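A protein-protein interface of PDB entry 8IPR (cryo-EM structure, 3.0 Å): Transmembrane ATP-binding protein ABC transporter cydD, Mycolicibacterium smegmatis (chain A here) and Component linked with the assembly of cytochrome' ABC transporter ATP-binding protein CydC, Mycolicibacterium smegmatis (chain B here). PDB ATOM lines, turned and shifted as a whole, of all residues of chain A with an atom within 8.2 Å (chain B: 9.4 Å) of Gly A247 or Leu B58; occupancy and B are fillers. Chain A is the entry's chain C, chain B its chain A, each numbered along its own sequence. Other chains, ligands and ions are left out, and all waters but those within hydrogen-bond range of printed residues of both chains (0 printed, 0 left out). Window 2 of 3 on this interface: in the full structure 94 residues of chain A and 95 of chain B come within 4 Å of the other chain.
Among the printed residues, merely in contact across the chains: Ala A240 with Arg B66 (3.8 Å), Val A244 with Val B62 (3.6 Å), Gly A247 with Leu B58 (3.5 Å), Leu A248 with Leu B58 (3.6 Å), Val A251 with Val B55 (3.7 Å) and Phe A252 with Val B55 (3.8 Å).
Ala A243 touches none of the printed residues of chain B. No residue of chain B comes within 4 Å of Val A246. Printed residues of chain B within 4 Å of Leu A248: Leu B58. Gly A260 touches none of the printed residues of chain B. Of the printed residues of chain A, Leu B58 touches Gly A247 and Leu A248. Of the printed residues of chain A, Arg B66 touches Ala A240 (3.8 Å). The nearest residue of chain B that does not touch Gly A247 is Val B55 (6.8 Å). The nearest printed residue of chain A that does not touch Arg B66 is Leu A241 (6.8 Å).
Hydrophobic or aromatic side chains of chain A within 4 Å of the printed part of chain B: Ala A240, Val A244, Val A251 and Phe A252. Among the printed residues, no Asp or Glu carboxylate lies within 4 Å of a Lys or Arg side-chain nitrogen of the other chain.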
ATOM      1  N   ALA A 240     -11.474 -18.163 -13.119  1.00  0.00           N
ATOM      2  CA  ALA A 240     -12.802 -18.030 -12.530  1.00  0.00           C
ATOM      3  C   ALA A 240     -13.690 -19.219 -12.859  1.00  0.00           C
ATOM      4  O   ALA A 240     -14.567 -19.574 -12.064  1.00  0.00           O
ATOM      5  CB  ALA A 240     -13.458 -16.734 -13.005  1.00  0.00           C
ATOM      6  N   LEU A 241     -13.459 -19.825 -14.026  1.00  0.00           N
ATOM      7  CA  LEU A 241     -14.229 -21.023 -14.460  1.00  0.00           C
ATOM      8  C   LEU A 241     -14.052 -22.132 -13.418  1.00  0.00           C
ATOM      9  O   LEU A 241     -15.076 -22.627 -12.904  1.00  0.00           O
ATOM     10  CB  LEU A 241     -13.717 -21.448 -15.840  1.00  0.00           C
ATOM     11  CG  LEU A 241     -14.336 -22.712 -16.437  1.00  0.00           C
ATOM     12  CD1 LEU A 241     -15.826 -22.528 -16.674  1.00  0.00           C
ATOM     13  CD2 LEU A 241     -13.634 -23.093 -17.730  1.00  0.00           C
ATOM     14  N   VAL A 242     -12.805 -22.493 -13.110  1.00  0.00           N
ATOM     15  CA  VAL A 242     -12.528 -23.542 -12.132  1.00  0.00           C
ATOM     16  C   VAL A 242     -12.901 -23.086 -10.727  1.00  0.00           C
ATOM     17  O   VAL A 242     -13.267 -23.911  -9.878  1.00  0.00           O
ATOM     18  CB  VAL A 242     -11.058 -23.999 -12.213  1.00  0.00           C
ATOM     19  CG1 VAL A 242     -10.158 -23.115 -11.368  1.00  0.00           C
ATOM     20  CG2 VAL A 242     -10.936 -25.444 -11.763  1.00  0.00           C
ATOM     21  N   ALA A 243     -12.823 -21.781 -10.452  1.00  0.00           N
ATOM     22  CA  ALA A 243     -13.263 -21.281  -9.154  1.00  0.00           C
ATOM     23  C   ALA A 243     -14.744 -21.564  -8.942  1.00  0.00           C
ATOM     24  O   ALA A 243     -15.151 -22.042  -7.879  1.00  0.00           O
ATOM     25  CB  ALA A 243     -12.977 -19.784  -9.043  1.00  0.00           C
ATOM     26  N   VAL A 244     -15.548 -21.262  -9.964  1.00  0.00           N
ATOM     27  CA  VAL A 244     -17.008 -21.567  -9.912  1.00  0.00           C
ATOM     28  C   VAL A 244     -17.183 -23.071  -9.695  1.00  0.00           C
ATOM     29  O   VAL A 244     -17.926 -23.451  -8.768  1.00  0.00           O
ATOM     30  CB  VAL A 244     -17.719 -21.099 -11.196  1.00  0.00           C
ATOM     31  CG1 VAL A 244     -19.184 -21.505 -11.223  1.00  0.00           C
ATOM     32  CG2 VAL A 244     -17.574 -19.600 -11.402  1.00  0.00           C
ATOM     33  N   SER A 245     -16.499 -23.890 -10.498  1.00  0.00           N
ATOM     34  CA  SER A 245     -16.681 -25.337 -10.412  1.00  0.00           C
ATOM     35  C   SER A 245     -16.418 -25.846  -8.998  1.00  0.00           C
ATOM     36  O   SER A 245     -17.252 -26.549  -8.409  1.00  0.00           O
ATOM     37  CB  SER A 245     -15.767 -26.040 -11.414  1.00  0.00           C
ATOM     38  OG  SER A 245     -15.893 -27.448 -11.318  1.00  0.00           O
ATOM     39  N   VAL A 246     -15.268 -25.484  -8.428  1.00  0.00           N
ATOM     40  CA  VAL A 246     -14.913 -25.995  -7.108  1.00  0.00           C
ATOM     41  C   VAL A 246     -15.823 -25.404  -6.036  1.00  0.00           C
ATOM     42  O   VAL A 246     -16.190 -26.089  -5.078  1.00  0.00           O
ATOM     43  CB  VAL A 246     -13.426 -25.735  -6.806  1.00  0.00           C
ATOM     44  CG1 VAL A 246     -13.177 -25.754  -5.307  1.00  0.00           C
ATOM     45  CG2 VAL A 246     -12.559 -26.771  -7.502  1.00  0.00           C
ATOM     46  N   GLY A 247     -16.207 -24.132  -6.174  1.00  0.00           N
ATOM     47  CA  GLY A 247     -17.120 -23.549  -5.206  1.00  0.00           C
ATOM     48  C   GLY A 247     -18.459 -24.258  -5.171  1.00  0.00           C
ATOM     49  O   GLY A 247     -18.999 -24.534  -4.095  1.00  0.00           O
ATOM     50  N   LEU A 248     -19.014 -24.567  -6.346  1.00  0.00           N
ATOM     51  CA  LEU A 248     -20.258 -25.329  -6.387  1.00  0.00           C
ATOM     52  C   LEU A 248     -20.071 -26.720  -5.798  1.00  0.00           C
ATOM     53  O   LEU A 248     -20.917 -27.193  -5.031  1.00  0.00           O
ATOM     54  CB  LEU A 248     -20.778 -25.421  -7.821  1.00  0.00           C
ATOM     55  CG  LEU A 248     -21.390 -24.144  -8.392  1.00  0.00           C
ATOM     56  CD1 LEU A 248     -21.722 -24.328  -9.858  1.00  0.00           C
ATOM     57  CD2 LEU A 248     -22.629 -23.755  -7.603  1.00  0.00           C
ATOM     58  N   ARG A 249     -18.967 -27.390  -6.134  1.00  0.00           N
ATOM     59  CA  ARG A 249     -18.757 -28.735  -5.609  1.00  0.00           C
ATOM     60  C   ARG A 249     -18.441 -28.735  -4.117  1.00  0.00           C
ATOM     61  O   ARG A 249     -18.528 -29.788  -3.478  1.00  0.00           O
ATOM     62  CB  ARG A 249     -17.645 -29.435  -6.389  1.00  0.00           C
ATOM     63  CG  ARG A 249     -18.016 -30.837  -6.832  1.00  0.00           C
ATOM     64  CD  ARG A 249     -16.814 -31.610  -7.336  1.00  0.00           C
ATOM     65  NE  ARG A 249     -15.854 -30.746  -8.011  1.00  0.00           N
ATOM     66  CZ  ARG A 249     -14.557 -31.003  -8.109  1.00  0.00           C
ATOM     67  NH1 ARG A 249     -14.033 -32.106  -7.601  1.00  0.00           N
ATOM     68  NH2 ARG A 249     -13.769 -30.135  -8.735  1.00  0.00           N
ATOM     69  N   LEU A 250     -18.072 -27.585  -3.556  1.00  0.00           N
ATOM     70  CA  LEU A 250     -17.789 -27.467  -2.131  1.00  0.00           C
ATOM     71  C   LEU A 250     -19.003 -27.049  -1.317  1.00  0.00           C
ATOM     72  O   LEU A 250     -19.121 -27.447  -0.153  1.00  0.00           O
ATOM     73  CB  LEU A 250     -16.660 -26.457  -1.901  1.00  0.00           C
ATOM     74  CG  LEU A 250     -15.388 -26.962  -1.220  1.00  0.00           C
ATOM     75  CD1 LEU A 250     -14.445 -25.805  -0.939  1.00  0.00           C
ATOM     76  CD2 LEU A 250     -15.725 -27.703   0.062  1.00  0.00           C
ATOM     77  N   VAL A 251     -19.898 -26.244  -1.894  1.00  0.00           N
ATOM     78  CA  VAL A 251     -21.089 -25.820  -1.163  1.00  0.00           C
ATOM     79  C   VAL A 251     -21.953 -27.023  -0.810  1.00  0.00           C
ATOM     80  O   VAL A 251     -22.458 -27.138   0.314  1.00  0.00           O
ATOM     81  CB  VAL A 251     -21.875 -24.774  -1.976  1.00  0.00           C
ATOM     82  CG1 VAL A 251     -23.312 -24.689  -1.489  1.00  0.00           C
ATOM     83  CG2 VAL A 251     -21.200 -23.416  -1.880  1.00  0.00           C
ATOM     84  N   PHE A 252     -22.126 -27.944  -1.754  1.00  0.00           N
ATOM     85  CA  PHE A 252     -22.942 -29.129  -1.529  1.00  0.00           C
ATOM     86  C   PHE A 252     -22.188 -30.250  -0.825  1.00  0.00           C
ATOM     87  O   PHE A 252     -22.791 -31.286  -0.527  1.00  0.00           O
ATOM     88  CB  PHE A 252     -23.508 -29.629  -2.861  1.00  0.00           C
ATOM     89  CG  PHE A 252     -24.355 -28.612  -3.574  1.00  0.00           C
ATOM     90  CD1 PHE A 252     -25.614 -28.285  -3.100  1.00  0.00           C
ATOM     91  CD2 PHE A 252     -23.890 -27.974  -4.710  1.00  0.00           C
ATOM     92  CE1 PHE A 252     -26.393 -27.349  -3.750  1.00  0.00           C
ATOM     93  CE2 PHE A 252     -24.663 -27.038  -5.365  1.00  0.00           C
ATOM     94  CZ  PHE A 252     -25.917 -26.724  -4.885  1.00  0.00           C
ATOM     95  N   GLY A 253     -20.895 -30.075  -0.555  1.00  0.00           N
ATOM     96  CA  GLY A 253     -20.161 -31.029   0.254  1.00  0.00           C
ATOM     97  C   GLY A 253     -19.613 -32.233  -0.474  1.00  0.00           C
ATOM     98  O   GLY A 253     -19.343 -33.254   0.165  1.00  0.00           O
ATOM     99  N   ASP A 254     -19.437 -32.154  -1.793  1.00  0.00           N
ATOM    100  CA  ASP A 254     -18.933 -33.300  -2.540  1.00  0.00           C
ATOM    101  C   ASP A 254     -17.438 -33.517  -2.338  1.00  0.00           C
ATOM    102  O   ASP A 254     -16.969 -34.659  -2.413  1.00  0.00           O
ATOM    103  CB  ASP A 254     -19.236 -33.131  -4.029  1.00  0.00           C
ATOM    104  CG  ASP A 254     -18.757 -34.306  -4.858  1.00  0.00           C
ATOM    105  OD1 ASP A 254     -19.479 -35.323  -4.921  1.00  0.00           O
ATOM    106  OD2 ASP A 254     -17.659 -34.214  -5.444  1.00  0.00           O
ATOM    107  N   MET A 255     -16.680 -32.456  -2.076  1.00  0.00           N
ATOM    108  CA  MET A 255     -15.229 -32.523  -2.012  1.00  0.00           C
ATOM    109  C   MET A 255     -14.720 -32.066  -0.650  1.00  0.00           C
ATOM    110  O   MET A 255     -15.425 -31.402   0.114  1.00  0.00           O
ATOM    111  CB  MET A 255     -14.586 -31.662  -3.104  1.00  0.00           C
ATOM    112  CG  MET A 255     -14.540 -30.186  -2.754  1.00  0.00           C
ATOM    113  SD  MET A 255     -13.198 -29.298  -3.557  1.00  0.00           S
ATOM    114  CE  MET A 255     -13.137 -30.127  -5.136  1.00  0.00           C
ATOM    115  N   GLY A 260     -10.076 -28.206  -2.163  1.00  0.00           N
ATOM    116  CA  GLY A 260     -10.642 -27.032  -2.806  1.00  0.00           C
ATOM    117  C   GLY A 260      -9.731 -25.824  -2.718  1.00  0.00           C
ATOM    118  O   GLY A 260      -9.506 -25.125  -3.712  1.00  0.00           O
ATOM    119  N   LEU A 264      -7.896 -23.902  -5.862  1.00  0.00           N
ATOM    120  CA  LEU A 264      -8.064 -22.465  -6.073  1.00  0.00           C
ATOM    121  C   LEU A 264      -6.729 -21.733  -6.047  1.00  0.00           C
ATOM    122  O   LEU A 264      -6.529 -20.775  -6.801  1.00  0.00           O
ATOM    123  CB  LEU A 264      -9.016 -21.870  -5.035  1.00  0.00           C
ATOM    124  CG  LEU A 264     -10.525 -21.931  -5.292  1.00  0.00           C
ATOM    125  CD1 LEU A 264     -10.939 -23.198  -6.003  1.00  0.00           C
ATOM    126  CD2 LEU A 264     -11.296 -21.771  -3.988  1.00  0.00           C
ATOM    127  N   SER B  42     -19.297  -6.886  -0.189  1.00  0.00           N
ATOM    128  CA  SER B  42     -19.739  -8.242   0.127  1.00  0.00           C
ATOM    129  C   SER B  42     -18.852  -8.855   1.203  1.00  0.00           C
ATOM    130  O   SER B  42     -18.294  -9.941   1.038  1.00  0.00           O
ATOM    131  CB  SER B  42     -19.755  -9.118  -1.121  1.00  0.00           C
ATOM    132  OG  SER B  42     -18.441  -9.411  -1.561  1.00  0.00           O
ATOM    133  N   LEU B  45     -22.402 -12.427   4.591  1.00  0.00           N
ATOM    134  CA  LEU B  45     -23.804 -12.550   4.211  1.00  0.00           C
ATOM    135  C   LEU B  45     -24.672 -11.609   5.039  1.00  0.00           C
ATOM    136  O   LEU B  45     -25.701 -12.022   5.584  1.00  0.00           O
ATOM    137  CB  LEU B  45     -24.285 -13.995   4.388  1.00  0.00           C
ATOM    138  CG  LEU B  45     -23.969 -15.060   3.329  1.00  0.00           C
ATOM    139  CD1 LEU B  45     -22.478 -15.172   3.031  1.00  0.00           C
ATOM    140  CD2 LEU B  45     -24.534 -16.410   3.750  1.00  0.00           C
ATOM    141  N   MET B  52     -28.821 -14.404   2.067  1.00  0.00           N
ATOM    142  CA  MET B  52     -29.019 -15.062   0.748  1.00  0.00           C
ATOM    143  C   MET B  52     -28.548 -16.518   0.824  1.00  0.00           C
ATOM    144  O   MET B  52     -27.633 -16.803   1.621  1.00  0.00           O
ATOM    145  CB  MET B  52     -28.230 -14.331  -0.342  1.00  0.00           C
ATOM    146  CG  MET B  52     -28.730 -12.926  -0.609  1.00  0.00           C
ATOM    147  SD  MET B  52     -30.457 -12.906  -1.149  1.00  0.00           S
ATOM    148  CE  MET B  52     -30.308 -13.711  -2.743  1.00  0.00           C
ATOM    149  N   PRO B  53     -29.137 -17.453   0.045  1.00  0.00           N
ATOM    150  CA  PRO B  53     -28.671 -18.842   0.017  1.00  0.00           C
ATOM    151  C   PRO B  53     -27.189 -18.915  -0.373  1.00  0.00           C
ATOM    152  O   PRO B  53     -26.754 -18.098  -1.168  1.00  0.00           O
ATOM    153  CB  PRO B  53     -29.511 -19.482  -1.096  1.00  0.00           C
ATOM    154  CG  PRO B  53     -30.764 -18.638  -1.144  1.00  0.00           C
ATOM    155  CD  PRO B  53     -30.296 -17.234  -0.822  1.00  0.00           C
ATOM    156  N   PRO B  54     -26.402 -19.883   0.147  1.00  0.00           N
ATOM    157  CA  PRO B  54     -24.956 -19.922  -0.149  1.00  0.00           C
ATOM    158  C   PRO B  54     -24.604 -19.902  -1.630  1.00  0.00           C
ATOM    159  O   PRO B  54     -23.616 -19.259  -2.007  1.00  0.00           O
ATOM    160  CB  PRO B  54     -24.498 -21.229   0.516  1.00  0.00           C
ATOM    161  CG  PRO B  54     -25.555 -21.568   1.505  1.00  0.00           C
ATOM    162  CD  PRO B  54     -26.837 -21.019   0.976  1.00  0.00           C
ATOM    163  N   VAL B  55     -25.366 -20.591  -2.482  1.00  0.00           N
ATOM    164  CA  VAL B  55     -25.015 -20.635  -3.900  1.00  0.00           C
ATOM    165  C   VAL B  55     -25.205 -19.264  -4.543  1.00  0.00           C
ATOM    166  O   VAL B  55     -24.416 -18.848  -5.403  1.00  0.00           O
ATOM    167  CB  VAL B  55     -25.818 -21.737  -4.620  1.00  0.00           C
ATOM    168  CG1 VAL B  55     -25.625 -23.069  -3.916  1.00  0.00           C
ATOM    169  CG2 VAL B  55     -27.298 -21.395  -4.680  1.00  0.00           C
ATOM    170  N   LEU B  56     -26.242 -18.535  -4.124  1.00  0.00           N
ATOM    171  CA  LEU B  56     -26.439 -17.172  -4.601  1.00  0.00           C
ATOM    172  C   LEU B  56     -25.272 -16.281  -4.196  1.00  0.00           C
ATOM    173  O   LEU B  56     -24.782 -15.478  -4.999  1.00  0.00           O
ATOM    174  CB  LEU B  56     -27.758 -16.623  -4.058  1.00  0.00           C
ATOM    175  CG  LEU B  56     -29.027 -16.930  -4.859  1.00  0.00           C
ATOM    176  CD1 LEU B  56     -29.396 -18.404  -4.814  1.00  0.00           C
ATOM    177  CD2 LEU B  56     -30.186 -16.080  -4.362  1.00  0.00           C
ATOM    178  N   ASP B  57     -24.806 -16.421  -2.952  1.00  0.00           N
ATOM    179  CA  ASP B  57     -23.660 -15.644  -2.494  1.00  0.00           C
ATOM    180  C   ASP B  57     -22.408 -15.990  -3.289  1.00  0.00           C
ATOM    181  O   ASP B  57     -21.619 -15.102  -3.630  1.00  0.00           O
ATOM    182  CB  ASP B  57     -23.428 -15.881  -1.003  1.00  0.00           C
ATOM    183  CG  ASP B  57     -24.300 -15.002  -0.134  1.00  0.00           C
ATOM    184  OD1 ASP B  57     -23.989 -13.801   0.005  1.00  0.00           O
ATOM    185  OD2 ASP B  57     -25.297 -15.516   0.414  1.00  0.00           O
ATOM    186  N   LEU B  58     -22.203 -17.274  -3.583  1.00  0.00           N
ATOM    187  CA  LEU B  58     -21.040 -17.680  -4.366  1.00  0.00           C
ATOM    188  C   LEU B  58     -21.076 -17.068  -5.761  1.00  0.00           C
ATOM    189  O   LEU B  58     -20.069 -16.540  -6.249  1.00  0.00           O
ATOM    190  CB  LEU B  58     -20.976 -19.206  -4.449  1.00  0.00           C
ATOM    191  CG  LEU B  58     -20.044 -19.797  -5.508  1.00  0.00           C
ATOM    192  CD1 LEU B  58     -18.597 -19.413  -5.240  1.00  0.00           C
ATOM    193  CD2 LEU B  58     -20.201 -21.305  -5.575  1.00  0.00           C
ATOM    194  N   THR B  59     -22.239 -17.125  -6.416  1.00  0.00           N
ATOM    195  CA  THR B  59     -22.361 -16.546  -7.751  1.00  0.00           C
ATOM    196  C   THR B  59     -22.129 -15.039  -7.720  1.00  0.00           C
ATOM    197  O   THR B  59     -21.423 -14.491  -8.579  1.00  0.00           O
ATOM    198  CB  THR B  59     -23.734 -16.875  -8.339  1.00  0.00           C
ATOM    199  OG1 THR B  59     -23.714 -18.198  -8.890  1.00  0.00           O
ATOM    200  CG2 THR B  59     -24.109 -15.885  -9.433  1.00  0.00           C
ATOM    201  N   VAL B  60     -22.703 -14.354  -6.725  1.00  0.00           N
ATOM    202  CA  VAL B  60     -22.522 -12.910  -6.610  1.00  0.00           C
ATOM    203  C   VAL B  60     -21.055 -12.569  -6.383  1.00  0.00           C
ATOM    204  O   VAL B  60     -20.519 -11.631  -6.987  1.00  0.00           O
ATOM    205  CB  VAL B  60     -23.418 -12.347  -5.490  1.00  0.00           C
ATOM    206  CG1 VAL B  60     -22.999 -10.932  -5.127  1.00  0.00           C
ATOM    207  CG2 VAL B  60     -24.878 -12.375  -5.917  1.00  0.00           C
ATOM    208  N   ALA B  61     -20.379 -13.323  -5.513  1.00  0.00           N
ATOM    209  CA  ALA B  61     -18.970 -13.063  -5.250  1.00  0.00           C
ATOM    210  C   ALA B  61     -18.129 -13.259  -6.503  1.00  0.00           C
ATOM    211  O   ALA B  61     -17.252 -12.438  -6.805  1.00  0.00           O
ATOM    212  CB  ALA B  61     -18.471 -13.965  -4.122  1.00  0.00           C
ATOM    213  N   VAL B  62     -18.385 -14.333  -7.253  1.00  0.00           N
ATOM    214  CA  VAL B  62     -17.600 -14.594  -8.458  1.00  0.00           C
ATOM    215  C   VAL B  62     -17.813 -13.489  -9.486  1.00  0.00           C
ATOM    216  O   VAL B  62     -16.855 -12.979 -10.085  1.00  0.00           O
ATOM    217  CB  VAL B  62     -17.942 -15.977  -9.039  1.00  0.00           C
ATOM    218  CG1 VAL B  62     -17.288 -16.147 -10.399  1.00  0.00           C
ATOM    219  CG2 VAL B  62     -17.489 -17.075  -8.093  1.00  0.00           C
ATOM    220  N   VAL B  63     -19.072 -13.094  -9.705  1.00  0.00           N
ATOM    221  CA  VAL B  63     -19.338 -12.082 -10.724  1.00  0.00           C
ATOM    222  C   VAL B  63     -18.761 -10.733 -10.303  1.00  0.00           C
ATOM    223  O   VAL B  63     -18.222  -9.992 -11.134  1.00  0.00           O
ATOM    224  CB  VAL B  63     -20.846 -12.003 -11.042  1.00  0.00           C
ATOM    225  CG1 VAL B  63     -21.645 -11.492  -9.861  1.00  0.00           C
ATOM    226  CG2 VAL B  63     -21.086 -11.126 -12.260  1.00  0.00           C
ATOM    227  N   ALA B  64     -18.832 -10.404  -9.008  1.00  0.00           N
ATOM    228  CA  ALA B  64     -18.251  -9.153  -8.534  1.00  0.00           C
ATOM    229  C   ALA B  64     -16.737  -9.148  -8.695  1.00  0.00           C
ATOM    230  O   ALA B  64     -16.156  -8.141  -9.122  1.00  0.00           O
ATOM    231  CB  ALA B  64     -18.637  -8.916  -7.074  1.00  0.00           C
ATOM    232  N   VAL B  65     -16.081 -10.263  -8.363  1.00  0.00           N
ATOM    233  CA  VAL B  65     -14.630 -10.341  -8.501  1.00  0.00           C
ATOM    234  C   VAL B  65     -14.225 -10.191  -9.961  1.00  0.00           C
ATOM    235  O   VAL B  65     -13.281  -9.458 -10.287  1.00  0.00           O
ATOM    236  CB  VAL B  65     -14.109 -11.659  -7.897  1.00  0.00           C
ATOM    237  CG1 VAL B  65     -12.745 -12.010  -8.468  1.00  0.00           C
ATOM    238  CG2 VAL B  65     -14.048 -11.557  -6.381  1.00  0.00           C
ATOM    239  N   ARG B  66     -14.933 -10.873 -10.864  1.00  0.00           N
ATOM    240  CA  ARG B  66     -14.594 -10.773 -12.280  1.00  0.00           C
ATOM    241  C   ARG B  66     -14.829  -9.363 -12.816  1.00  0.00           C
ATOM    242  O   ARG B  66     -14.024  -8.852 -13.604  1.00  0.00           O
ATOM    243  CB  ARG B  66     -15.385 -11.799 -13.085  1.00  0.00           C
ATOM    244  CG  ARG B  66     -14.687 -13.141 -13.212  1.00  0.00           C
ATOM    245  CD  ARG B  66     -13.421 -13.021 -14.043  1.00  0.00           C
ATOM    246  NE  ARG B  66     -13.702 -12.911 -15.471  1.00  0.00           N
ATOM    247  CZ  ARG B  66     -13.088 -12.074 -16.296  1.00  0.00           C
ATOM    248  NH1 ARG B  66     -12.154 -11.242 -15.868  1.00  0.00           N
ATOM    249  NH2 ARG B  66     -13.423 -12.070 -17.582  1.00  0.00           N
